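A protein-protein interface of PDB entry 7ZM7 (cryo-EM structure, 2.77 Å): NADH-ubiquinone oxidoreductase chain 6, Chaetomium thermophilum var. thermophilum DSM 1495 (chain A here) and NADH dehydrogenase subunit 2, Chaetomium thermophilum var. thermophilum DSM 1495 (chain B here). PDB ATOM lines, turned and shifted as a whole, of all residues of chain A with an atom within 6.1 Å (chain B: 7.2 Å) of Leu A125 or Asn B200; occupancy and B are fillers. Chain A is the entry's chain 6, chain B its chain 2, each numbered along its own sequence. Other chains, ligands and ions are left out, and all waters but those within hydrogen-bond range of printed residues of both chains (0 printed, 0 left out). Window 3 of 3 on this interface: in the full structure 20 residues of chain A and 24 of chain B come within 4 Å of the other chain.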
ATOM      1  N   LEU A 121       0.968  22.645   6.174  1.00  0.00           N
ATOM      2  CA  LEU A 121       1.944  21.975   5.323  1.00  0.00           C
ATOM      3  C   LEU A 121       1.834  20.460   5.407  1.00  0.00           C
ATOM      4  O   LEU A 121       2.094  19.771   4.416  1.00  0.00           O
ATOM      5  CB  LEU A 121       3.355  22.419   5.689  1.00  0.00           C
ATOM      6  CG  LEU A 121       3.957  23.551   4.858  1.00  0.00           C
ATOM      7  CD1 LEU A 121       5.184  24.119   5.543  1.00  0.00           C
ATOM      8  CD2 LEU A 121       4.310  23.049   3.469  1.00  0.00           C
ATOM      9  N   PHE A 122       1.436  19.909   6.555  1.00  0.00           N
ATOM     10  CA  PHE A 122       1.414  18.426   6.690  1.00  0.00           C
ATOM     11  C   PHE A 122       0.424  17.813   5.695  1.00  0.00           C
ATOM     12  O   PHE A 122       0.732  16.740   5.144  1.00  0.00           O
ATOM     13  CB  PHE A 122       1.050  18.033   8.123  1.00  0.00           C
ATOM     14  CG  PHE A 122       1.041  16.552   8.403  1.00  0.00           C
ATOM     15  CD1 PHE A 122       2.213  15.880   8.705  1.00  0.00           C
ATOM     16  CD2 PHE A 122      -0.143  15.832   8.380  1.00  0.00           C
ATOM     17  CE1 PHE A 122       2.203  14.520   8.968  1.00  0.00           C
ATOM     18  CE2 PHE A 122      -0.153  14.471   8.640  1.00  0.00           C
ATOM     19  CZ  PHE A 122       1.021  13.818   8.935  1.00  0.00           C
ATOM     20  N   LYS A 123      -0.709  18.474   5.453  1.00  0.00           N
ATOM     21  CA  LYS A 123      -1.704  17.975   4.464  1.00  0.00           C
ATOM     22  C   LYS A 123      -1.053  17.924   3.083  1.00  0.00           C
ATOM     23  O   LYS A 123      -1.433  17.053   2.288  1.00  0.00           O
ATOM     24  CB  LYS A 123      -2.945  18.869   4.464  1.00  0.00           C
ATOM     25  CG  LYS A 123      -3.664  18.966   5.802  1.00  0.00           C
ATOM     26  CD  LYS A 123      -4.299  17.660   6.227  1.00  0.00           C
ATOM     27  CE  LYS A 123      -4.662  17.632   7.696  1.00  0.00           C
ATOM     28  NZ  LYS A 123      -3.469  17.826   8.554  1.00  0.00           N
ATOM     29  N   MET A 124      -0.120  18.751   2.779  1.00  0.00           N
ATOM     30  CA  MET A 124       0.495  18.797   1.428  1.00  0.00           C
ATOM     31  C   MET A 124       1.417  17.613   1.175  1.00  0.00           C
ATOM     32  O   MET A 124       1.631  17.304   0.004  1.00  0.00           O
ATOM     33  CB  MET A 124       1.291  20.088   1.267  1.00  0.00           C
ATOM     34  CG  MET A 124       0.357  21.232   1.052  1.00  0.00           C
ATOM     35  SD  MET A 124      -0.910  20.794  -0.163  1.00  0.00           S
ATOM     36  CE  MET A 124      -2.400  21.128   0.776  1.00  0.00           C
ATOM     37  N   LEU A 125       1.992  17.056   2.152  1.00  0.00           N
ATOM     38  CA  LEU A 125       2.960  15.970   1.952  1.00  0.00           C
ATOM     39  C   LEU A 125       2.261  14.784   1.268  1.00  0.00           C
ATOM     40  O   LEU A 125       1.062  14.600   1.532  1.00  0.00           O
ATOM     41  CB  LEU A 125       3.557  15.587   3.308  1.00  0.00           C
ATOM     42  CG  LEU A 125       4.302  16.700   4.040  1.00  0.00           C
ATOM     43  CD1 LEU A 125       4.562  16.315   5.488  1.00  0.00           C
ATOM     44  CD2 LEU A 125       5.608  17.033   3.336  1.00  0.00           C
ATOM     45  N   PRO A 126       2.896  13.929   0.529  1.00  0.00           N
ATOM     46  CA  PRO A 126       2.272  12.740  -0.089  1.00  0.00           C
ATOM     47  C   PRO A 126       2.119  11.531   0.853  1.00  0.00           C
ATOM     48  O   PRO A 126       2.686  11.560   1.930  1.00  0.00           O
ATOM     49  CB  PRO A 126       3.290  12.434  -1.178  1.00  0.00           C
ATOM     50  CG  PRO A 126       4.606  12.759  -0.543  1.00  0.00           C
ATOM     51  CD  PRO A 126       4.317  14.025   0.228  1.00  0.00           C
ATOM     52  N   TYR A 127       1.347  10.518   0.462  1.00  0.00           N
ATOM     53  CA  TYR A 127       1.077   9.360   1.358  1.00  0.00           C
ATOM     54  C   TYR A 127       2.340   8.567   1.701  1.00  0.00           C
ATOM     55  O   TYR A 127       2.459   8.129   2.858  1.00  0.00           O
ATOM     56  CB  TYR A 127       0.037   8.422   0.756  1.00  0.00           C
ATOM     57  CG  TYR A 127      -0.732   7.652   1.797  1.00  0.00           C
ATOM     58  CD1 TYR A 127      -1.541   8.311   2.705  1.00  0.00           C
ATOM     59  CD2 TYR A 127      -0.651   6.271   1.881  1.00  0.00           C
ATOM     60  CE1 TYR A 127      -2.257   7.622   3.669  1.00  0.00           C
ATOM     61  CE2 TYR A 127      -1.362   5.568   2.839  1.00  0.00           C
ATOM     62  CZ  TYR A 127      -2.166   6.245   3.736  1.00  0.00           C
ATOM     63  OH  TYR A 127      -2.870   5.564   4.686  1.00  0.00           O
ATOM     64  N   VAL A 129       5.370   9.453   2.248  1.00  0.00           N
ATOM     65  CA  VAL A 129       6.280  10.092   3.247  1.00  0.00           C
ATOM     66  C   VAL A 129       5.685   9.946   4.652  1.00  0.00           C
ATOM     67  O   VAL A 129       6.468   9.759   5.603  1.00  0.00           O
ATOM     68  CB  VAL A 129       6.529  11.568   2.883  1.00  0.00           C
ATOM     69  CG1 VAL A 129       7.182  12.352   4.011  1.00  0.00           C
ATOM     70  CG2 VAL A 129       7.348  11.689   1.608  1.00  0.00           C
ATOM     71  N   ILE A 130       4.354   9.965   4.773  1.00  0.00           N
ATOM     72  CA  ILE A 130       3.704   9.844   6.074  1.00  0.00           C
ATOM     73  C   ILE A 130       3.171   8.432   6.277  1.00  0.00           C
ATOM     74  O   ILE A 130       2.259   8.212   7.081  1.00  0.00           O
ATOM     75  CB  ILE A 130       2.574  10.878   6.232  1.00  0.00           C
ATOM     76  CG1 ILE A 130       1.516  10.689   5.144  1.00  0.00           C
ATOM     77  CG2 ILE A 130       3.133  12.285   6.197  1.00  0.00           C
ATOM     78  CD1 ILE A 130       0.296  11.560   5.327  1.00  0.00           C
ATOM     79  N   THR B 194       8.461  24.481  -5.146  1.00  0.00           N
ATOM     80  CA  THR B 194       8.783  23.550  -6.219  1.00  0.00           C
ATOM     81  C   THR B 194       8.942  22.135  -5.694  1.00  0.00           C
ATOM     82  O   THR B 194       8.522  21.178  -6.342  1.00  0.00           O
ATOM     83  CB  THR B 194      10.055  23.999  -6.921  1.00  0.00           C
ATOM     84  OG1 THR B 194      11.070  24.217  -5.946  1.00  0.00           O
ATOM     85  CG2 THR B 194       9.823  25.269  -7.670  1.00  0.00           C
ATOM     86  N   SER B 195       9.549  21.985  -4.519  1.00  0.00           N
ATOM     87  CA  SER B 195       9.719  20.664  -3.933  1.00  0.00           C
ATOM     88  C   SER B 195       8.374  19.994  -3.684  1.00  0.00           C
ATOM     89  O   SER B 195       8.194  18.814  -3.991  1.00  0.00           O
ATOM     90  CB  SER B 195      10.502  20.775  -2.633  1.00  0.00           C
ATOM     91  OG  SER B 195       9.667  21.226  -1.587  1.00  0.00           O
ATOM     92  N   LEU B 196       7.418  20.733  -3.124  1.00  0.00           N
ATOM     93  CA  LEU B 196       6.099  20.184  -2.874  1.00  0.00           C
ATOM     94  C   LEU B 196       5.331  19.918  -4.148  1.00  0.00           C
ATOM     95  O   LEU B 196       4.357  19.166  -4.127  1.00  0.00           O
ATOM     96  CB  LEU B 196       5.299  21.123  -1.987  1.00  0.00           C
ATOM     97  CG  LEU B 196       5.645  21.064  -0.516  1.00  0.00           C
ATOM     98  CD1 LEU B 196       4.988  22.219   0.099  1.00  0.00           C
ATOM     99  CD2 LEU B 196       5.140  19.796   0.068  1.00  0.00           C
ATOM    100  N   LEU B 197       5.744  20.520  -5.253  1.00  0.00           N
ATOM    101  CA  LEU B 197       5.151  20.187  -6.535  1.00  0.00           C
ATOM    102  C   LEU B 197       5.604  18.819  -7.011  1.00  0.00           C
ATOM    103  O   LEU B 197       4.775  17.972  -7.343  1.00  0.00           O
ATOM    104  CB  LEU B 197       5.515  21.253  -7.559  1.00  0.00           C
ATOM    105  CG  LEU B 197       4.595  22.457  -7.581  1.00  0.00           C
ATOM    106  CD1 LEU B 197       5.280  23.580  -8.300  1.00  0.00           C
ATOM    107  CD2 LEU B 197       3.300  22.099  -8.247  1.00  0.00           C
ATOM    108  N   TYR B 198       6.916  18.597  -7.060  1.00  0.00           N
ATOM    109  CA  TYR B 198       7.460  17.342  -7.568  1.00  0.00           C
ATOM    110  C   TYR B 198       7.076  16.173  -6.670  1.00  0.00           C
ATOM    111  O   TYR B 198       6.698  15.103  -7.147  1.00  0.00           O
ATOM    112  CB  TYR B 198       8.984  17.478  -7.712  1.00  0.00           C
ATOM    113  CG  TYR B 198       9.742  16.183  -7.751  1.00  0.00           C
ATOM    114  CD1 TYR B 198       9.824  15.440  -8.919  1.00  0.00           C
ATOM    115  CD2 TYR B 198      10.366  15.699  -6.620  1.00  0.00           C
ATOM    116  CE1 TYR B 198      10.494  14.261  -8.960  1.00  0.00           C
ATOM    117  CE2 TYR B 198      11.042  14.506  -6.649  1.00  0.00           C
ATOM    118  CZ  TYR B 198      11.104  13.794  -7.826  1.00  0.00           C
ATOM    119  OH  TYR B 198      11.788  12.611  -7.855  1.00  0.00           O
ATOM    120  N   VAL B 199       7.066  16.406  -5.367  1.00  0.00           N
ATOM    121  CA  VAL B 199       6.805  15.339  -4.359  1.00  0.00           C
ATOM    122  C   VAL B 199       5.349  14.849  -4.401  1.00  0.00           C
ATOM    123  O   VAL B 199       5.063  13.791  -3.842  1.00  0.00           O
ATOM    124  CB  VAL B 199       7.283  15.870  -2.993  1.00  0.00           C
ATOM    125  CG1 VAL B 199       6.451  15.508  -1.788  1.00  0.00           C
ATOM    126  CG2 VAL B 199       8.774  15.697  -2.765  1.00  0.00           C
ATOM    127  N   ASN B 200       4.467  15.575  -5.082  1.00  0.00           N
ATOM    128  CA  ASN B 200       3.043  15.172  -5.153  1.00  0.00           C
ATOM    129  C   ASN B 200       2.683  14.761  -6.569  1.00  0.00           C
ATOM    130  O   ASN B 200       1.730  14.010  -6.724  1.00  0.00           O
ATOM    131  CB  ASN B 200       2.138  16.301  -4.691  1.00  0.00           C
ATOM    132  CG  ASN B 200       2.073  16.445  -3.185  1.00  0.00           C
ATOM    133  OD1 ASN B 200       1.590  15.555  -2.495  1.00  0.00           O
ATOM    134  ND2 ASN B 200       2.532  17.569  -2.667  1.00  0.00           N
ATOM    135  N   SER B 201       3.445  15.215  -7.556  1.00  0.00           N
ATOM    136  CA  SER B 201       3.142  14.957  -8.979  1.00  0.00           C
ATOM    137  C   SER B 201       4.152  14.013  -9.625  1.00  0.00           C
ATOM    138  O   SER B 201       3.886  13.595 -10.745  1.00  0.00           O
ATOM    139  CB  SER B 201       3.150  16.261  -9.663  1.00  0.00           C
ATOM    140  OG  SER B 201       4.437  16.840  -9.606  1.00  0.00           O
ATOM    141  N   GLY B 202       5.297  13.752  -8.997  1.00  0.00           N
ATOM    142  CA  GLY B 202       6.309  12.938  -9.633  1.00  0.00           C
ATOM    143  C   GLY B 202       6.990  13.538 -10.836  1.00  0.00           C
ATOM    144  O   GLY B 202       7.778  12.856 -11.480  1.00  0.00           O
ATOM    145  N   THR B 203       6.708  14.803 -11.133  1.00  0.00           N
ATOM    146  CA  THR B 203       7.257  15.440 -12.351  1.00  0.00           C
ATOM    147  C   THR B 203       7.896  16.781 -12.020  1.00  0.00           C
ATOM    148  O   THR B 203       7.480  17.384 -11.026  1.00  0.00           O
ATOM    149  CB  THR B 203       6.167  15.664 -13.410  1.00  0.00           C
ATOM    150  OG1 THR B 203       6.786  16.204 -14.579  1.00  0.00           O
ATOM    151  CG2 THR B 203       5.039  16.564 -12.960  1.00  0.00           C
ATOM    152  N   LEU B 209       2.631  19.182 -15.293  1.00  0.00           N
ATOM    153  CA  LEU B 209       1.834  19.799 -14.206  1.00  0.00           C
ATOM    154  C   LEU B 209       0.625  20.515 -14.800  1.00  0.00           C
ATOM    155  O   LEU B 209      -0.442  20.455 -14.178  1.00  0.00           O
ATOM    156  CB  LEU B 209       2.732  20.799 -13.481  1.00  0.00           C
ATOM    157  CG  LEU B 209       3.658  20.203 -12.422  1.00  0.00           C
ATOM    158  CD1 LEU B 209       4.709  21.213 -11.990  1.00  0.00           C
ATOM    159  CD2 LEU B 209       2.862  19.715 -11.223  1.00  0.00           C
ATOM    160  N   LEU B 212      -1.852  17.774 -15.691  1.00  0.00           N
ATOM    161  CA  LEU B 212      -2.458  17.207 -14.460  1.00  0.00           C
ATOM    162  C   LEU B 212      -3.497  18.198 -13.939  1.00  0.00           C
ATOM    163  O   LEU B 212      -4.521  17.743 -13.433  1.00  0.00           O
ATOM    164  CB  LEU B 212      -1.355  16.932 -13.431  1.00  0.00           C
ATOM    165  CG  LEU B 212      -0.443  15.745 -13.719  1.00  0.00           C
ATOM    166  CD1 LEU B 212       0.675  15.674 -12.691  1.00  0.00           C
ATOM    167  CD2 LEU B 212      -1.234  14.451 -13.734  1.00  0.00           C
ATOM    168  N   TYR B 235      -7.667  11.222  -4.996  1.00  0.00           N
ATOM    169  CA  TYR B 235      -6.471  12.097  -5.114  1.00  0.00           C
ATOM    170  C   TYR B 235      -6.856  13.481  -5.628  1.00  0.00           C
ATOM    171  O   TYR B 235      -6.644  13.755  -6.811  1.00  0.00           O
ATOM    172  CB  TYR B 235      -5.437  11.482  -6.055  1.00  0.00           C
ATOM    173  CG  TYR B 235      -4.748  10.252  -5.530  1.00  0.00           C
ATOM    174  CD1 TYR B 235      -5.242   8.987  -5.799  1.00  0.00           C
ATOM    175  CD2 TYR B 235      -3.598  10.356  -4.769  1.00  0.00           C
ATOM    176  CE1 TYR B 235      -4.616   7.853  -5.317  1.00  0.00           C
ATOM    177  CE2 TYR B 235      -2.951   9.231  -4.288  1.00  0.00           C
ATOM    178  CZ  TYR B 235      -3.466   7.977  -4.560  1.00  0.00           C
ATOM    179  OH  TYR B 235      -2.829   6.871  -4.090  1.00  0.00           O
ATOM    180  N   TYR B 239      -2.722  20.256  -4.005  1.00  0.00           N
ATOM    181  CA  TYR B 239      -1.315  20.683  -3.898  1.00  0.00           C
ATOM    182  C   TYR B 239      -0.983  21.766  -4.908  1.00  0.00           C
ATOM    183  O   TYR B 239      -0.213  22.625  -4.530  1.00  0.00           O
ATOM    184  CB  TYR B 239      -0.391  19.478  -4.089  1.00  0.00           C
ATOM    185  CG  TYR B 239      -0.336  18.886  -5.473  1.00  0.00           C
ATOM    186  CD1 TYR B 239      -1.296  17.989  -5.907  1.00  0.00           C
ATOM    187  CD2 TYR B 239       0.695  19.203  -6.342  1.00  0.00           C
ATOM    188  CE1 TYR B 239      -1.248  17.443  -7.176  1.00  0.00           C
ATOM    189  CE2 TYR B 239       0.754  18.669  -7.618  1.00  0.00           C
ATOM    190  CZ  TYR B 239      -0.219  17.782  -8.032  1.00  0.00           C
ATOM    191  OH  TYR B 239      -0.169  17.245  -9.284  1.00  0.00           O
ATOM    192  N   LEU B 240      -1.511  21.711  -6.130  1.00  0.00           N
ATOM    193  CA  LEU B 240      -1.079  22.677  -7.159  1.00  0.00           C
ATOM    194  C   LEU B 240      -1.324  24.108  -6.675  1.00  0.00           C
ATOM    195  O   LEU B 240      -0.411  24.919  -6.781  1.00  0.00           O
ATOM    196  CB  LEU B 240      -1.807  22.371  -8.463  1.00  0.00           C
ATOM    197  CG  LEU B 240      -1.426  23.275  -9.633  1.00  0.00           C
ATOM    198  CD1 LEU B 240      -0.160  22.781 -10.315  1.00  0.00           C
ATOM    199  CD2 LEU B 240      -2.565  23.393 -10.629  1.00  0.00           C
ATOM    200  N   SER B 243       0.903  24.700  -3.476  1.00  0.00           N
ATOM    201  CA  SER B 243       2.310  24.814  -3.835  1.00  0.00           C
ATOM    202  C   SER B 243       2.604  26.129  -4.531  1.00  0.00           C
ATOM    203  O   SER B 243       3.612  26.777  -4.241  1.00  0.00           O
ATOM    204  CB  SER B 243       2.720  23.650  -4.725  1.00  0.00           C
ATOM    205  OG  SER B 243       2.701  22.446  -4.002  1.00  0.00           O
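Of the 16 printed residues of chain B, 4 touch a printed residue of chain A. Hydrophobic or aromatic side chains of chain B that line the printed part of chain A: Leu B196 and Val B199. Of the 9 printed residues of chain A, 4 touch a printed residue of chain B. Hydrophobic or aromatic side chains of chain A within 4 Å of the printed part of chain B: Leu A121, Met A124 and Pro A126. Along chain A the printed residues that touch a printed residue of chain B span positions 121 to 126. Among the printed residues, no Asp or Glu carboxylate lies within 4 Å of a Lys or Arg side-chain nitrogen of the other chain.
Of the printed residues of chain B, Leu A121 touches Leu B196. Of chain B, only Asn B200 comes within 4 Å of Leu A125. Of the printed residues of chain A, Leu B196 touches Leu A121 (3.5 Å). Printed residues of chain A within 4 Å of Val B199: Pro A126. Asn B200 touches just these residues of chain A: Met A124, Leu A125 and Pro A126. Of the printed residues of chain A, Tyr B239 touches Met A124. The nearest residue of chain B that does not touch Leu A125 is Leu B196 (4.3 Å). The nearest printed residue of chain B that does not touch Leu A121 is Asn B200 (7.4 Å).
Among the printed residues, merely in contact across the chains: Pro A126 with Val B199 (3.3 Å), Leu A121 with Leu B196 (3.5 Å), Pro A126 with Asn B200 (3.7 Å), Met A124 with Tyr B239 (3.8 Å) and Leu A125 with Asn B200 (3.9 Å).
ND2 of Asn B200 sits at hydrogen-bond distance from O of Leu B196 (2.8 Å). The side-chain hydroxyl of Ser B243 sits at hydrogen-bond distance from the backbone carbonyl oxygen of Tyr B239, 3.0 Å away.
O of Met A124 sits at hydrogen-bond distance from ND2 of Asn B200, at 2.8 Å.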
